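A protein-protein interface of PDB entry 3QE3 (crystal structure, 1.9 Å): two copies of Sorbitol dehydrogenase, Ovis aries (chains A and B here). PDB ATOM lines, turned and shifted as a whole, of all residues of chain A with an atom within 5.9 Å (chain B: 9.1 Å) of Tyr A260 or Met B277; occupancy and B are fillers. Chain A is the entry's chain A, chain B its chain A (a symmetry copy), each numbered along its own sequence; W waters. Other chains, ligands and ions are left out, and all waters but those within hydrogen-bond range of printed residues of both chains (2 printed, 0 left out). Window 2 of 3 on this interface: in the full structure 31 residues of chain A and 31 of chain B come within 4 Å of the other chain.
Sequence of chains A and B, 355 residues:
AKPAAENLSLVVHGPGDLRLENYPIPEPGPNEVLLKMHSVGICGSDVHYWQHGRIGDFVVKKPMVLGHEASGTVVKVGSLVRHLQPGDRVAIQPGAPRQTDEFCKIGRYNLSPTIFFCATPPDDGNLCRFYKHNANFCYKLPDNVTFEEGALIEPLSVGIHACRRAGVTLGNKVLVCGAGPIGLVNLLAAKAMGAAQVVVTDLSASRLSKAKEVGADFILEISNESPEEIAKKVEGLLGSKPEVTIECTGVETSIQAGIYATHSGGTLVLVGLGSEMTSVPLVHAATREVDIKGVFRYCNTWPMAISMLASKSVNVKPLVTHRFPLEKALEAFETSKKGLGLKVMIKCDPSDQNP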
ATOM      1  N   PRO A 227      21.474  26.287  22.507  1.00  0.00           N
ATOM      2  CA  PRO A 227      22.428  25.394  21.832  1.00  0.00           C
ATOM      3  C   PRO A 227      23.604  24.995  22.733  1.00  0.00           C
ATOM      4  O   PRO A 227      24.037  23.844  22.691  1.00  0.00           O
ATOM      5  CB  PRO A 227      22.902  26.236  20.637  1.00  0.00           C
ATOM      6  CG  PRO A 227      21.725  27.150  20.355  1.00  0.00           C
ATOM      7  CD  PRO A 227      21.200  27.505  21.719  1.00  0.00           C
ATOM      8  N   GLU A 228      24.098  25.923  23.549  1.00  0.00           N
ATOM      9  CA  GLU A 228      25.197  25.618  24.460  1.00  0.00           C
ATOM     10  C   GLU A 228      24.795  24.607  25.531  1.00  0.00           C
ATOM     11  O   GLU A 228      25.594  23.741  25.906  1.00  0.00           O
ATOM     12  CB  GLU A 228      25.733  26.885  25.121  1.00  0.00           C
ATOM     13  CG  GLU A 228      26.478  27.832  24.179  1.00  0.00           C
ATOM     14  CD  GLU A 228      25.565  28.877  23.551  1.00  0.00           C
ATOM     15  OE1 GLU A 228      24.328  28.675  23.567  1.00  0.00           O
ATOM     16  OE2 GLU A 228      26.085  29.900  23.047  1.00  0.00           O
ATOM     17  N   ALA A 231      24.512  21.118  23.872  1.00  0.00           N
ATOM     18  CA  ALA A 231      25.868  20.592  23.741  1.00  0.00           C
ATOM     19  C   ALA A 231      26.369  20.095  25.089  1.00  0.00           C
ATOM     20  O   ALA A 231      27.043  19.063  25.187  1.00  0.00           O
ATOM     21  CB  ALA A 231      26.834  21.664  23.158  1.00  0.00           C
ATOM     22  N   LYS A 241      32.940  15.060  24.486  1.00  0.00           N
ATOM     23  CA  LYS A 241      32.323  15.664  23.314  1.00  0.00           C
ATOM     24  C   LYS A 241      32.390  14.648  22.184  1.00  0.00           C
ATOM     25  O   LYS A 241      33.424  14.015  21.983  1.00  0.00           O
ATOM     26  CB  LYS A 241      33.049  16.956  22.922  1.00  0.00           C
ATOM     27  CG  LYS A 241      32.832  18.131  23.872  1.00  0.00           C
ATOM     28  CD  LYS A 241      33.085  19.443  23.132  1.00  0.00           C
ATOM     29  CE  LYS A 241      32.763  20.653  23.984  1.00  0.00           C
ATOM     30  NZ  LYS A 241      33.586  20.684  25.228  1.00  0.00           N
ATOM     31  N   ILE A 255      21.529  23.081  14.445  1.00  0.00           N
ATOM     32  CA  ILE A 255      22.817  23.236  13.774  1.00  0.00           C
ATOM     33  C   ILE A 255      23.825  23.922  14.711  1.00  0.00           C
ATOM     34  O   ILE A 255      24.946  23.459  14.885  1.00  0.00           O
ATOM     35  CB  ILE A 255      22.648  23.971  12.436  1.00  0.00           C
ATOM     36  CG1 ILE A 255      21.793  23.117  11.500  1.00  0.00           C
ATOM     37  CG2 ILE A 255      24.003  24.244  11.805  1.00  0.00           C
ATOM     38  CD1 ILE A 255      21.201  23.860  10.333  1.00  0.00           C
ATOM     39  N   GLN A 256      23.411  24.996  15.365  1.00  0.00           N
ATOM     40  CA  GLN A 256      24.288  25.646  16.329  1.00  0.00           C
ATOM     41  C   GLN A 256      24.694  24.708  17.454  1.00  0.00           C
ATOM     42  O   GLN A 256      25.853  24.700  17.872  1.00  0.00           O
ATOM     43  CB  GLN A 256      23.621  26.897  16.898  1.00  0.00           C
ATOM     44  CG  GLN A 256      23.198  27.873  15.825  1.00  0.00           C
ATOM     45  CD  GLN A 256      22.358  29.001  16.388  1.00  0.00           C
ATOM     46  OE1 GLN A 256      21.763  28.869  17.462  1.00  0.00           O
ATOM     47  NE2 GLN A 256      22.310  30.117  15.673  1.00  0.00           N
ATOM     48  N   ALA A 257      23.738  23.921  17.947  1.00  0.00           N
ATOM     49  CA  ALA A 257      24.015  22.947  18.997  1.00  0.00           C
ATOM     50  C   ALA A 257      25.124  22.002  18.561  1.00  0.00           C
ATOM     51  O   ALA A 257      26.071  21.750  19.305  1.00  0.00           O
ATOM     52  CB  ALA A 257      22.753  22.162  19.341  1.00  0.00           C
ATOM     53  N   GLY A 258      25.004  21.499  17.339  1.00  0.00           N
ATOM     54  CA  GLY A 258      26.014  20.620  16.764  1.00  0.00           C
ATOM     55  C   GLY A 258      27.408  21.229  16.768  1.00  0.00           C
ATOM     56  O   GLY A 258      28.395  20.554  17.062  1.00  0.00           O
ATOM     57  N   ILE A 259      27.491  22.513  16.447  1.00  0.00           N
ATOM     58  CA  ILE A 259      28.763  23.221  16.455  1.00  0.00           C
ATOM     59  C   ILE A 259      29.379  23.301  17.855  1.00  0.00           C
ATOM     60  O   ILE A 259      30.579  23.059  18.034  1.00  0.00           O
ATOM     61  CB  ILE A 259      28.605  24.621  15.815  1.00  0.00           C
ATOM     62  CG1 ILE A 259      28.218  24.445  14.338  1.00  0.00           C
ATOM     63  CG2 ILE A 259      29.873  25.442  16.006  1.00  0.00           C
ATOM     64  CD1 ILE A 259      28.117  25.727  13.528  1.00  0.00           C
ATOM     65  N   TYR A 260      28.561  23.620  18.854  1.00  0.00           N
ATOM     66  CA  TYR A 260      29.062  23.678  20.224  1.00  0.00           C
ATOM     67  C   TYR A 260      29.384  22.282  20.763  1.00  0.00           C
ATOM     68  O   TYR A 260      30.319  22.111  21.547  1.00  0.00           O
ATOM     69  CB  TYR A 260      28.068  24.384  21.148  1.00  0.00           C
ATOM     70  CG  TYR A 260      27.787  25.831  20.778  1.00  0.00           C
ATOM     71  CD1 TYR A 260      28.778  26.798  20.864  1.00  0.00           C
ATOM     72  CD2 TYR A 260      26.526  26.223  20.347  1.00  0.00           C
ATOM     73  CE1 TYR A 260      28.520  28.126  20.530  1.00  0.00           C
ATOM     74  CE2 TYR A 260      26.258  27.540  20.008  1.00  0.00           C
ATOM     75  CZ  TYR A 260      27.257  28.483  20.100  1.00  0.00           C
ATOM     76  OH  TYR A 260      26.977  29.783  19.760  1.00  0.00           O
ATOM     77  N   ALA A 261      28.611  21.290  20.324  1.00  0.00           N
ATOM     78  CA  ALA A 261      28.706  19.928  20.864  1.00  0.00           C
ATOM     79  C   ALA A 261      29.903  19.127  20.349  1.00  0.00           C
ATOM     80  O   ALA A 261      30.482  18.316  21.074  1.00  0.00           O
ATOM     81  CB  ALA A 261      27.397  19.164  20.598  1.00  0.00           C
ATOM     82  N   THR A 262      30.297  19.363  19.102  1.00  0.00           N
ATOM     83  CA  THR A 262      31.264  18.487  18.457  1.00  0.00           C
ATOM     84  C   THR A 262      32.692  18.661  18.995  1.00  0.00           C
ATOM     85  O   THR A 262      33.152  19.774  19.216  1.00  0.00           O
ATOM     86  CB  THR A 262      31.210  18.666  16.924  1.00  0.00           C
ATOM     87  OG1 THR A 262      29.867  18.428  16.482  1.00  0.00           O
ATOM     88  CG2 THR A 262      32.132  17.693  16.231  1.00  0.00           C
ATOM     89  N   SER A 279      22.215  31.179  10.287  1.00  0.00           N
ATOM     90  CA  SER A 279      23.065  31.958  11.179  1.00  0.00           C
ATOM     91  C   SER A 279      23.745  30.997  12.139  1.00  0.00           C
ATOM     92  O   SER A 279      23.075  30.295  12.897  1.00  0.00           O
ATOM     93  CB  SER A 279      22.228  32.974  11.969  1.00  0.00           C
ATOM     94  OG  SER A 279      23.028  33.667  12.920  1.00  0.00           O
ATOM     95  N   VAL A 280      25.073  30.967  12.104  1.00  0.00           N
ATOM     96  CA  VAL A 280      25.833  29.997  12.878  1.00  0.00           C
ATOM     97  C   VAL A 280      27.104  30.585  13.469  1.00  0.00           C
ATOM     98  O   VAL A 280      27.697  31.506  12.901  1.00  0.00           O
ATOM     99  CB  VAL A 280      26.210  28.771  12.013  1.00  0.00           C
ATOM    100  CG1 VAL A 280      24.997  27.854  11.816  1.00  0.00           C
ATOM    101  CG2 VAL A 280      26.790  29.223  10.668  1.00  0.00           C
ATOM    102  N   PRO A 281      27.525  30.060  14.626  1.00  0.00           N
ATOM    103  CA  PRO A 281      28.822  30.434  15.189  1.00  0.00           C
ATOM    104  C   PRO A 281      29.900  29.801  14.338  1.00  0.00           C
ATOM    105  O   PRO A 281      30.668  28.966  14.812  1.00  0.00           O
ATOM    106  CB  PRO A 281      28.796  29.798  16.585  1.00  0.00           C
ATOM    107  CG  PRO A 281      27.862  28.638  16.438  1.00  0.00           C
ATOM    108  CD  PRO A 281      26.798  29.111  15.491  1.00  0.00           C
ATOM    109  N   LEU A 282      29.929  30.205  13.073  1.00  0.00           N
ATOM    110  CA  LEU A 282      30.876  29.691  12.102  1.00  0.00           C
ATOM    111  C   LEU A 282      32.286  29.751  12.660  1.00  0.00           C
ATOM    112  O   LEU A 282      33.062  28.803  12.529  1.00  0.00           O
ATOM    113  CB  LEU A 282      30.783  30.511  10.817  1.00  0.00           C
ATOM    114  CG  LEU A 282      31.397  29.895   9.577  1.00  0.00           C
ATOM    115  CD1 LEU A 282      31.078  28.411   9.511  1.00  0.00           C
ATOM    116  CD2 LEU A 282      30.913  30.633   8.330  1.00  0.00           C
ATOM    117  N   HIS A 284      33.259  29.759  15.878  1.00  0.00           N
ATOM    118  CA  HIS A 284      33.456  28.768  16.938  1.00  0.00           C
ATOM    119  C   HIS A 284      33.919  27.421  16.367  1.00  0.00           C
ATOM    120  O   HIS A 284      34.914  26.839  16.814  1.00  0.00           O
ATOM    121  CB  HIS A 284      32.165  28.583  17.740  1.00  0.00           C
ATOM    122  CG  HIS A 284      32.340  27.769  18.983  1.00  0.00           C
ATOM    123  ND1 HIS A 284      31.974  26.442  19.062  1.00  0.00           N
ATOM    124  CD2 HIS A 284      32.849  28.090  20.195  1.00  0.00           C
ATOM    125  CE1 HIS A 284      32.247  25.982  20.270  1.00  0.00           C
ATOM    126  NE2 HIS A 284      32.777  26.962  20.978  1.00  0.00           N
ATOM    127  N   ARG A 288      38.070  25.662  16.128  1.00  0.00           N
ATOM    128  CA  ARG A 288      38.247  24.374  16.798  1.00  0.00           C
ATOM    129  C   ARG A 288      38.473  23.255  15.780  1.00  0.00           C
ATOM    130  O   ARG A 288      38.484  22.076  16.129  1.00  0.00           O
ATOM    131  CB  ARG A 288      37.033  24.058  17.679  1.00  0.00           C
ATOM    132  CG  ARG A 288      36.816  25.065  18.814  1.00  0.00           C
ATOM    133  CD  ARG A 288      35.529  24.776  19.591  1.00  0.00           C
ATOM    134  NE  ARG A 288      35.577  23.421  20.125  1.00  0.00           N
ATOM    135  CZ  ARG A 288      34.676  22.472  19.892  1.00  0.00           C
ATOM    136  NH1 ARG A 288      33.600  22.722  19.158  1.00  0.00           N
ATOM    137  NH2 ARG A 288      34.838  21.272  20.425  1.00  0.00           N
ATOM    138  N   GLY B 250      37.653  37.264   6.526  1.00  0.00           N
ATOM    139  CA  GLY B 250      36.712  37.186   7.634  1.00  0.00           C
ATOM    140  C   GLY B 250      35.430  37.963   7.389  1.00  0.00           C
ATOM    141  O   GLY B 250      34.586  38.084   8.273  1.00  0.00           O
ATOM    142  N   VAL B 251      35.268  38.487   6.183  1.00  0.00           N
ATOM    143  CA  VAL B 251      34.111  39.314   5.872  1.00  0.00           C
ATOM    144  C   VAL B 251      32.951  38.485   5.323  1.00  0.00           C
ATOM    145  O   VAL B 251      33.099  37.779   4.318  1.00  0.00           O
ATOM    146  CB  VAL B 251      34.484  40.453   4.895  1.00  0.00           C
ATOM    147  CG1 VAL B 251      33.232  41.150   4.378  1.00  0.00           C
ATOM    148  CG2 VAL B 251      35.405  41.446   5.588  1.00  0.00           C
ATOM    149  N   GLU B 252      31.794  38.590   5.982  1.00  0.00           N
ATOM    150  CA  GLU B 252      30.665  37.703   5.721  1.00  0.00           C
ATOM    151  C   GLU B 252      30.332  37.576   4.244  1.00  0.00           C
ATOM    152  O   GLU B 252      30.154  36.468   3.735  1.00  0.00           O
ATOM    153  CB  GLU B 252      29.423  38.140   6.515  1.00  0.00           C
ATOM    154  CG  GLU B 252      28.142  37.441   6.076  1.00  0.00           C
ATOM    155  CD  GLU B 252      26.977  37.710   7.013  1.00  0.00           C
ATOM    156  OE1 GLU B 252      27.111  37.416   8.221  1.00  0.00           O
ATOM    157  OE2 GLU B 252      25.935  38.219   6.541  1.00  0.00           O
ATOM    158  N   ILE B 255      32.765  35.361   2.579  1.00  0.00           N
ATOM    159  CA  ILE B 255      32.464  33.970   2.905  1.00  0.00           C
ATOM    160  C   ILE B 255      31.323  33.450   2.015  1.00  0.00           C
ATOM    161  O   ILE B 255      31.421  32.386   1.415  1.00  0.00           O
ATOM    162  CB  ILE B 255      32.171  33.814   4.405  1.00  0.00           C
ATOM    163  CG1 ILE B 255      33.429  34.163   5.201  1.00  0.00           C
ATOM    164  CG2 ILE B 255      31.733  32.392   4.716  1.00  0.00           C
ATOM    165  CD1 ILE B 255      33.193  34.458   6.657  1.00  0.00           C
ATOM    166  N   GLY B 274      36.074  36.218  11.393  1.00  0.00           N
ATOM    167  CA  GLY B 274      34.829  36.940  11.192  1.00  0.00           C
ATOM    168  C   GLY B 274      34.147  37.300  12.499  1.00  0.00           C
ATOM    169  O   GLY B 274      34.757  37.241  13.568  1.00  0.00           O
ATOM    170  N   SER B 275      32.878  37.683  12.412  1.00  0.00           N
ATOM    171  CA  SER B 275      32.086  37.993  13.597  1.00  0.00           C
ATOM    172  C   SER B 275      31.630  36.705  14.292  1.00  0.00           C
ATOM    173  O   SER B 275      31.716  35.626  13.711  1.00  0.00           O
ATOM    174  CB  SER B 275      30.885  38.865  13.224  1.00  0.00           C
ATOM    175  OG  SER B 275      30.290  38.422  12.013  1.00  0.00           O
ATOM    176  N   GLU B 276      31.161  36.825  15.532  1.00  0.00           N
ATOM    177  CA  GLU B 276      30.768  35.667  16.331  1.00  0.00           C
ATOM    178  C   GLU B 276      29.690  34.851  15.641  1.00  0.00           C
ATOM    179  O   GLU B 276      29.657  33.630  15.744  1.00  0.00           O
ATOM    180  CB  GLU B 276      30.283  36.104  17.713  1.00  0.00           C
ATOM    181  CG  GLU B 276      31.385  36.626  18.620  1.00  0.00           C
ATOM    182  CD  GLU B 276      32.398  35.554  18.989  1.00  0.00           C
ATOM    183  OE1 GLU B 276      32.514  35.241  20.194  1.00  0.00           O
ATOM    184  OE2 GLU B 276      33.081  35.031  18.082  1.00  0.00           O
ATOM    185  N   MET B 277      28.806  35.534  14.935  1.00  0.00           N
ATOM    186  CA  MET B 277      27.769  34.859  14.183  1.00  0.00           C
ATOM    187  C   MET B 277      27.939  35.193  12.725  1.00  0.00           C
ATOM    188  O   MET B 277      28.155  36.354  12.366  1.00  0.00           O
ATOM    189  CB  MET B 277      26.384  35.326  14.625  1.00  0.00           C
ATOM    190  CG  MET B 277      25.960  34.863  15.986  1.00  0.00           C
ATOM    191  SD  MET B 277      25.691  33.088  16.066  1.00  0.00           S
ATOM    192  CE  MET B 277      27.004  32.685  17.220  1.00  0.00           C
ATOM    193  N   THR B 278      27.829  34.184  11.875  1.00  0.00           N
ATOM    194  CA  THR B 278      27.869  34.438  10.455  1.00  0.00           C
ATOM    195  C   THR B 278      26.590  33.958   9.802  1.00  0.00           C
ATOM    196  O   THR B 278      26.039  32.924  10.175  1.00  0.00           O
ATOM    197  CB  THR B 278      29.067  33.753   9.809  1.00  0.00           C
ATOM    198  OG1 THR B 278      30.202  33.870  10.683  1.00  0.00           O
ATOM    199  CG2 THR B 278      29.362  34.383   8.470  1.00  0.00           C
ATOM    200  N   SER B 279      26.131  34.715   8.816  1.00  0.00           N
ATOM    201  CA  SER B 279      24.955  34.344   8.038  1.00  0.00           C
ATOM    202  C   SER B 279      25.426  33.863   6.676  1.00  0.00           C
ATOM    203  O   SER B 279      26.055  34.617   5.933  1.00  0.00           O
ATOM    204  CB  SER B 279      24.019  35.548   7.869  1.00  0.00           C
ATOM    205  OG  SER B 279      22.921  35.229   7.021  1.00  0.00           O
ATOM    206  N   VAL B 280      25.122  32.610   6.353  1.00  0.00           N
ATOM    207  CA  VAL B 280      25.628  31.993   5.137  1.00  0.00           C
ATOM    208  C   VAL B 280      24.601  31.100   4.461  1.00  0.00           C
ATOM    209  O   VAL B 280      23.739  30.516   5.123  1.00  0.00           O
ATOM    210  CB  VAL B 280      26.897  31.158   5.426  1.00  0.00           C
ATOM    211  CG1 VAL B 280      28.114  32.070   5.622  1.00  0.00           C
ATOM    212  CG2 VAL B 280      26.677  30.255   6.646  1.00  0.00           C
HETATM  213  O   HOH W   1      31.005  33.133  13.121  1.00  0.00           O
HETATM  214  O   HOH W   2      31.635  31.858  17.212  1.00  0.00           O
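The backbone carbonyl oxygen of Val A280 sits at hydrogen-bond distance from the backbone NH of Thr B278 (2.9 Å).
OE2 of Glu A228 sits at hydrogen-bond distance from OH of Tyr A260 (3.4 Å).
The side-chain amide nitrogen of Gln A256 sits at hydrogen-bond distance from the backbone carbonyl oxygen of Ser A279, 2.9 Å away.
The side-chain hydroxyl of Ser B275 sits at hydrogen-bond distance from the backbone carbonyl oxygen of Met B277, 3.0 Å away.
Met B277 touches Tyr A260 (CE to OH, 3.9 Å).
Ser A279 touches Thr B278.
Met B277 touches Val A280.
O of Glu B276 touches CA of Pro A281, 3.3 Å away.
CB of Pro A281 touches CE of Met B277 (3.5 Å).
OG1 of Thr B278 touches CB of Leu A282, 3.4 Å away.
Tyr A260 touches just one residue of chain B: Met B277 (3.9 Å).
Of chain A, only Tyr A260 (3.9 Å), Val A280 (3.6 Å) and Pro A281 (3.5 Å) come within 4 Å of Met B277.
No residue of chain B comes within 4 Å of Gly A258.
No residue of chain B comes within 4 Å of Ala A261.
Of the printed residues of chain B, Ser A279 touches Thr B278.
Of the printed residues of chain B, Pro A281 touches Glu B276 (3.3 Å) and Met B277 (3.5 Å).
Pro A227 touches none of the printed residues of chain B.
Val B280 touches none of the printed residues of chain A.
Hydrophobic or aromatic side chains of chain B within 4 Å of the printed part of chain A: Met B277.
Positions printed for both chains: 255, 279 and 280.
Water W1 lies within hydrogen-bond range of O of Ser B275 (2.7 Å), OG1 of Thr B278 (2.7 Å), O of Glu B276 (3.0 Å) and N of Leu A282 (3.1 Å).
Water W2 lies within hydrogen-bond range of the backbone NH (N) of His A284 and the backbone carbonyl oxygen (O) of Glu B276.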
